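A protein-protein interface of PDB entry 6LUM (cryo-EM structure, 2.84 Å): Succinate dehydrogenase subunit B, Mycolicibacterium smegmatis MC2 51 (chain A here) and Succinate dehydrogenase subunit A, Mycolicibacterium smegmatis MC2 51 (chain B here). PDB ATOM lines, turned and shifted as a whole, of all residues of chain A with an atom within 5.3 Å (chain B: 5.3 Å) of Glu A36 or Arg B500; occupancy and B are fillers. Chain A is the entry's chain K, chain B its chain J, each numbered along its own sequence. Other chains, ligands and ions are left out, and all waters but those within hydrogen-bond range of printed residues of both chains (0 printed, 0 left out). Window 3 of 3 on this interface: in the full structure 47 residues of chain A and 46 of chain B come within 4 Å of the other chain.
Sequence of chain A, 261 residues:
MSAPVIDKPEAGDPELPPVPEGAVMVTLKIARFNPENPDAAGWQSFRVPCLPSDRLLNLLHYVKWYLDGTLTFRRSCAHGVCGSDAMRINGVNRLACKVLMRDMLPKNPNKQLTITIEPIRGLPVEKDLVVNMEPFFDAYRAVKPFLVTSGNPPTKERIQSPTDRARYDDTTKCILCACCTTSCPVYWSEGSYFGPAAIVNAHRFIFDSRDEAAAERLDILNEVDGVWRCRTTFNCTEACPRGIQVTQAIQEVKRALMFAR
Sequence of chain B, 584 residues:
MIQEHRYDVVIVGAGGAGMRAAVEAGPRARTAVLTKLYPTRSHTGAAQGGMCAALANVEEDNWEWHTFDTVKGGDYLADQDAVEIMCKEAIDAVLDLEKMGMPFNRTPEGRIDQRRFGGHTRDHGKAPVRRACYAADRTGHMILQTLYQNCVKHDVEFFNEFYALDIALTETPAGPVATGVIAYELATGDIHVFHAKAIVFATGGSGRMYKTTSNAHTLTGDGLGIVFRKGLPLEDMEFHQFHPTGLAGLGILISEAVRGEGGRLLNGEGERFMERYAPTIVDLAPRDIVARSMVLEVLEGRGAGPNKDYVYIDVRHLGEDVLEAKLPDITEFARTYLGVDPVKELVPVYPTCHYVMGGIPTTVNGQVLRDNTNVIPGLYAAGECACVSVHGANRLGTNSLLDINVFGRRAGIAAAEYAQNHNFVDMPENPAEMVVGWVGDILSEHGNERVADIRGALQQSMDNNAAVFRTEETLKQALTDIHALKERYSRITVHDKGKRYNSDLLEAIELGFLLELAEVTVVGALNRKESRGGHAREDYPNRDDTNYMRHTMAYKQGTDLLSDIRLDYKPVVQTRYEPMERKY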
ATOM      1  N   ASN A  34       7.823  20.025  16.373  1.00  0.00           N
ATOM      2  CA  ASN A  34       6.773  20.352  17.326  1.00  0.00           C
ATOM      3  C   ASN A  34       5.534  20.787  16.569  1.00  0.00           C
ATOM      4  O   ASN A  34       5.629  21.669  15.711  1.00  0.00           O
ATOM      5  CB  ASN A  34       7.237  21.465  18.256  1.00  0.00           C
ATOM      6  CG  ASN A  34       6.677  21.338  19.654  1.00  0.00           C
ATOM      7  OD1 ASN A  34       5.802  20.523  19.918  1.00  0.00           O
ATOM      8  ND2 ASN A  34       7.197  22.143  20.566  1.00  0.00           N
ATOM      9  N   PRO A  35       4.375  20.204  16.821  1.00  0.00           N
ATOM     10  CA  PRO A  35       3.218  20.487  15.969  1.00  0.00           C
ATOM     11  C   PRO A  35       2.553  21.814  16.264  1.00  0.00           C
ATOM     12  O   PRO A  35       1.867  22.361  15.396  1.00  0.00           O
ATOM     13  CB  PRO A  35       2.273  19.325  16.282  1.00  0.00           C
ATOM     14  CG  PRO A  35       2.584  18.989  17.670  1.00  0.00           C
ATOM     15  CD  PRO A  35       4.059  19.193  17.839  1.00  0.00           C
ATOM     16  N   GLU A  36       2.712  22.334  17.475  1.00  0.00           N
ATOM     17  CA  GLU A  36       2.040  23.582  17.805  1.00  0.00           C
ATOM     18  C   GLU A  36       2.959  24.663  18.344  1.00  0.00           C
ATOM     19  O   GLU A  36       2.790  25.827  17.978  1.00  0.00           O
ATOM     20  CB  GLU A  36       0.917  23.340  18.827  1.00  0.00           C
ATOM     21  CG  GLU A  36       1.394  22.951  20.213  1.00  0.00           C
ATOM     22  CD  GLU A  36       0.264  22.805  21.199  1.00  0.00           C
ATOM     23  OE1 GLU A  36      -0.904  22.939  20.782  1.00  0.00           O
ATOM     24  OE2 GLU A  36       0.543  22.578  22.392  1.00  0.00           O
ATOM     25  N   ASN A  37       3.920  24.330  19.207  1.00  0.00           N
ATOM     26  CA  ASN A  37       4.539  25.415  19.961  1.00  0.00           C
ATOM     27  C   ASN A  37       5.435  26.264  19.052  1.00  0.00           C
ATOM     28  O   ASN A  37       5.083  27.424  18.798  1.00  0.00           O
ATOM     29  CB  ASN A  37       5.255  24.859  21.197  1.00  0.00           C
ATOM     30  CG  ASN A  37       4.299  24.188  22.169  1.00  0.00           C
ATOM     31  OD1 ASN A  37       4.040  22.990  22.074  1.00  0.00           O
ATOM     32  ND2 ASN A  37       3.769  24.962  23.108  1.00  0.00           N
ATOM     33  N   PRO A  38       6.588  25.779  18.537  1.00  0.00           N
ATOM     34  CA  PRO A  38       7.023  26.279  17.229  1.00  0.00           C
ATOM     35  C   PRO A  38       6.680  25.294  16.129  1.00  0.00           C
ATOM     36  O   PRO A  38       6.705  24.085  16.366  1.00  0.00           O
ATOM     37  CB  PRO A  38       8.534  26.436  17.400  1.00  0.00           C
ATOM     38  CG  PRO A  38       8.893  25.323  18.280  1.00  0.00           C
ATOM     39  CD  PRO A  38       7.720  25.118  19.221  1.00  0.00           C
ATOM     40  N   ASP A  39       6.364  25.768  14.933  1.00  0.00           N
ATOM     41  CA  ASP A  39       6.456  24.903  13.759  1.00  0.00           C
ATOM     42  C   ASP A  39       7.798  25.088  13.066  1.00  0.00           C
ATOM     43  O   ASP A  39       7.883  25.300  11.859  1.00  0.00           O
ATOM     44  CB  ASP A  39       5.299  25.159  12.809  1.00  0.00           C
ATOM     45  CG  ASP A  39       3.989  24.636  13.349  1.00  0.00           C
ATOM     46  OD1 ASP A  39       4.026  23.687  14.153  1.00  0.00           O
ATOM     47  OD2 ASP A  39       2.922  25.158  12.968  1.00  0.00           O
ATOM     48  N   GLU A 126       2.979  13.744  13.245  1.00  0.00           N
ATOM     49  CA  GLU A 126       2.195  14.438  14.255  1.00  0.00           C
ATOM     50  C   GLU A 126       3.042  15.077  15.335  1.00  0.00           C
ATOM     51  O   GLU A 126       2.650  16.105  15.880  1.00  0.00           O
ATOM     52  CB  GLU A 126       1.201  13.477  14.908  1.00  0.00           C
ATOM     53  CG  GLU A 126       0.160  12.945  13.957  1.00  0.00           C
ATOM     54  CD  GLU A 126      -0.763  14.027  13.436  1.00  0.00           C
ATOM     55  OE1 GLU A 126      -1.847  14.220  14.020  1.00  0.00           O
ATOM     56  OE2 GLU A 126      -0.409  14.687  12.439  1.00  0.00           O
ATOM     57  N   LYS A 127       4.184  14.490  15.659  1.00  0.00           N
ATOM     58  CA  LYS A 127       5.182  15.076  16.535  1.00  0.00           C
ATOM     59  C   LYS A 127       6.494  14.388  16.195  1.00  0.00           C
ATOM     60  O   LYS A 127       6.580  13.671  15.194  1.00  0.00           O
ATOM     61  CB  LYS A 127       4.767  14.926  18.004  1.00  0.00           C
ATOM     62  CG  LYS A 127       5.328  15.982  18.922  1.00  0.00           C
ATOM     63  CD  LYS A 127       4.403  16.228  20.076  1.00  0.00           C
ATOM     64  CE  LYS A 127       5.076  17.049  21.139  1.00  0.00           C
ATOM     65  NZ  LYS A 127       6.351  16.438  21.565  1.00  0.00           N
ATOM     66  N   LEU B 186      -5.097  11.759  23.804  1.00  0.00           N
ATOM     67  CA  LEU B 186      -3.675  12.067  23.717  1.00  0.00           C
ATOM     68  C   LEU B 186      -3.378  12.951  22.522  1.00  0.00           C
ATOM     69  O   LEU B 186      -2.503  13.814  22.589  1.00  0.00           O
ATOM     70  CB  LEU B 186      -2.863  10.778  23.627  1.00  0.00           C
ATOM     71  CG  LEU B 186      -1.388  10.933  23.260  1.00  0.00           C
ATOM     72  CD1 LEU B 186      -0.554  11.299  24.457  1.00  0.00           C
ATOM     73  CD2 LEU B 186      -0.862   9.688  22.606  1.00  0.00           C
ATOM     74  N   ALA B 187      -4.112  12.765  21.427  1.00  0.00           N
ATOM     75  CA  ALA B 187      -3.774  13.419  20.170  1.00  0.00           C
ATOM     76  C   ALA B 187      -4.034  14.917  20.195  1.00  0.00           C
ATOM     77  O   ALA B 187      -3.358  15.668  19.488  1.00  0.00           O
ATOM     78  CB  ALA B 187      -4.558  12.783  19.028  1.00  0.00           C
ATOM     79  N   THR B 188      -5.018  15.376  20.966  1.00  0.00           N
ATOM     80  CA  THR B 188      -5.378  16.784  20.978  1.00  0.00           C
ATOM     81  C   THR B 188      -5.421  17.396  22.367  1.00  0.00           C
ATOM     82  O   THR B 188      -5.629  18.604  22.478  1.00  0.00           O
ATOM     83  CB  THR B 188      -6.744  17.001  20.320  1.00  0.00           C
ATOM     84  OG1 THR B 188      -7.754  16.382  21.118  1.00  0.00           O
ATOM     85  CG2 THR B 188      -6.774  16.394  18.936  1.00  0.00           C
ATOM     86  N   GLY B 189      -5.247  16.613  23.420  1.00  0.00           N
ATOM     87  CA  GLY B 189      -5.286  17.147  24.760  1.00  0.00           C
ATOM     88  C   GLY B 189      -6.665  17.472  25.283  1.00  0.00           C
ATOM     89  O   GLY B 189      -6.788  17.860  26.448  1.00  0.00           O
ATOM     90  N   GLY B 498       2.787  21.282  26.634  1.00  0.00           N
ATOM     91  CA  GLY B 498       2.029  21.328  25.406  1.00  0.00           C
ATOM     92  C   GLY B 498       0.695  20.637  25.552  1.00  0.00           C
ATOM     93  O   GLY B 498       0.302  20.188  26.625  1.00  0.00           O
ATOM     94  N   LYS B 499      -0.018  20.548  24.439  1.00  0.00           N
ATOM     95  CA  LYS B 499      -1.334  19.928  24.463  1.00  0.00           C
ATOM     96  C   LYS B 499      -1.589  19.036  23.259  1.00  0.00           C
ATOM     97  O   LYS B 499      -2.722  18.571  23.089  1.00  0.00           O
ATOM     98  CB  LYS B 499      -2.426  20.996  24.548  1.00  0.00           C
ATOM     99  CG  LYS B 499      -2.666  21.524  25.950  1.00  0.00           C
ATOM    100  CD  LYS B 499      -3.988  22.256  26.042  1.00  0.00           C
ATOM    101  CE  LYS B 499      -5.103  21.462  25.385  1.00  0.00           C
ATOM    102  NZ  LYS B 499      -6.443  22.058  25.618  1.00  0.00           N
ATOM    103  N   ARG B 500      -0.585  18.770  22.428  1.00  0.00           N
ATOM    104  CA  ARG B 500      -0.804  17.972  21.228  1.00  0.00           C
ATOM    105  C   ARG B 500      -0.528  16.491  21.471  1.00  0.00           C
ATOM    106  O   ARG B 500      -1.418  15.661  21.297  1.00  0.00           O
ATOM    107  CB  ARG B 500       0.053  18.507  20.083  1.00  0.00           C
ATOM    108  CG  ARG B 500      -0.368  19.873  19.586  1.00  0.00           C
ATOM    109  CD  ARG B 500      -1.769  19.868  19.014  1.00  0.00           C
ATOM    110  NE  ARG B 500      -1.965  18.784  18.062  1.00  0.00           N
ATOM    111  CZ  ARG B 500      -3.106  18.559  17.423  1.00  0.00           C
ATOM    112  NH1 ARG B 500      -4.150  19.346  17.634  1.00  0.00           N
ATOM    113  NH2 ARG B 500      -3.205  17.545  16.575  1.00  0.00           N
ATOM    114  N   TYR B 501       0.696  16.139  21.849  1.00  0.00           N
ATOM    115  CA  TYR B 501       1.018  14.757  22.220  1.00  0.00           C
ATOM    116  C   TYR B 501       1.873  14.846  23.475  1.00  0.00           C
ATOM    117  O   TYR B 501       3.102  14.822  23.402  1.00  0.00           O
ATOM    118  CB  TYR B 501       1.747  14.014  21.112  1.00  0.00           C
ATOM    119  CG  TYR B 501       0.866  13.376  20.080  1.00  0.00           C
ATOM    120  CD1 TYR B 501       0.388  14.101  19.014  1.00  0.00           C
ATOM    121  CD2 TYR B 501       0.532  12.042  20.161  1.00  0.00           C
ATOM    122  CE1 TYR B 501      -0.409  13.527  18.070  1.00  0.00           C
ATOM    123  CE2 TYR B 501      -0.266  11.457  19.220  1.00  0.00           C
ATOM    124  CZ  TYR B 501      -0.732  12.204  18.175  1.00  0.00           C
ATOM    125  OH  TYR B 501      -1.531  11.623  17.226  1.00  0.00           O
ATOM    126  N   ASN B 502       1.227  14.923  24.622  1.00  0.00           N
ATOM    127  CA  ASN B 502       1.924  15.110  25.880  1.00  0.00           C
ATOM    128  C   ASN B 502       2.120  13.742  26.515  1.00  0.00           C
ATOM    129  O   ASN B 502       1.146  13.031  26.774  1.00  0.00           O
ATOM    130  CB  ASN B 502       1.139  16.050  26.788  1.00  0.00           C
ATOM    131  CG  ASN B 502       2.029  16.873  27.676  1.00  0.00           C
ATOM    132  OD1 ASN B 502       3.233  16.663  27.721  1.00  0.00           O
ATOM    133  ND2 ASN B 502       1.447  17.828  28.375  1.00  0.00           N
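Among the printed residues, pairs that only touch across the chains: Glu A36 with Arg B500 (3.3 Å), Pro A35 with Arg B500 (3.5 Å), Glu A126 with Tyr B501 (3.5 Å), Glu A36 with Gly B498 (3.6 Å) and Lys A127 with Tyr B501 (3.6 Å).
Asn A34 touches none of the printed residues of chain B.
Of the printed residues of chain B, Pro A35 touches Arg B500.
Printed residues of chain B within 4 Å of Glu A36: Gly B498 (3.6 Å), Lys B499 (2.9 Å) and Arg B500 (3.3 Å).
Pro A38 touches none of the printed residues of chain B.
Of the printed residues of chain A, Lys B499 touches Glu A36 (2.9 Å).
Arg B500 touches just these residues of chain A: Pro A35 and Glu A36.
The nearest residue of chain A that does not touch Arg B500 is Glu A126 (4.4 Å).
The nearest printed residue of chain B that does not touch Pro A35 is Tyr B501 (5.4 Å).
O of Leu B186 sits close to O of Arg B500 (2.5 Å).
The guanidinium group (NH2) of Arg B500 sits at hydrogen-bond distance from the backbone carbonyl oxygen (O) of Ala B187, at 3.5 Å.
The backbone carbonyl oxygen of Lys B499 lies within hydrogen-bond range of the backbone NH of Gly B189 (3.2 Å).
ND2 of Asn B502 sits at hydrogen-bond distance from O of Gly B498, 3.2 Å away.
Hydrophobic or aromatic side chains of chain B that line the printed part of chain A: Tyr B501.
Along chain B the printed residues that touch a printed residue of chain A span positions 498 to 501.
Of the 8 printed residues of chain A, 4 touch a printed residue of chain B.
Printed residues of chain A that touch a printed residue of chain B: Pro A35, Glu A36, Glu A126 and Lys A127.
Hydrophobic or aromatic side chains of chain A that line the printed part of chain B: Pro A35.
Among the printed residues, 6 pairs touch across the chains.
Among the printed residues, no Asp or Glu carboxylate lies within 4 Å of a Lys or Arg side-chain nitrogen of the other chain.
The backbone NH (N) of Lys B499 sits at hydrogen-bond distance from the side-chain carboxylate (OE2) of Glu A36, 2.9 Å away.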
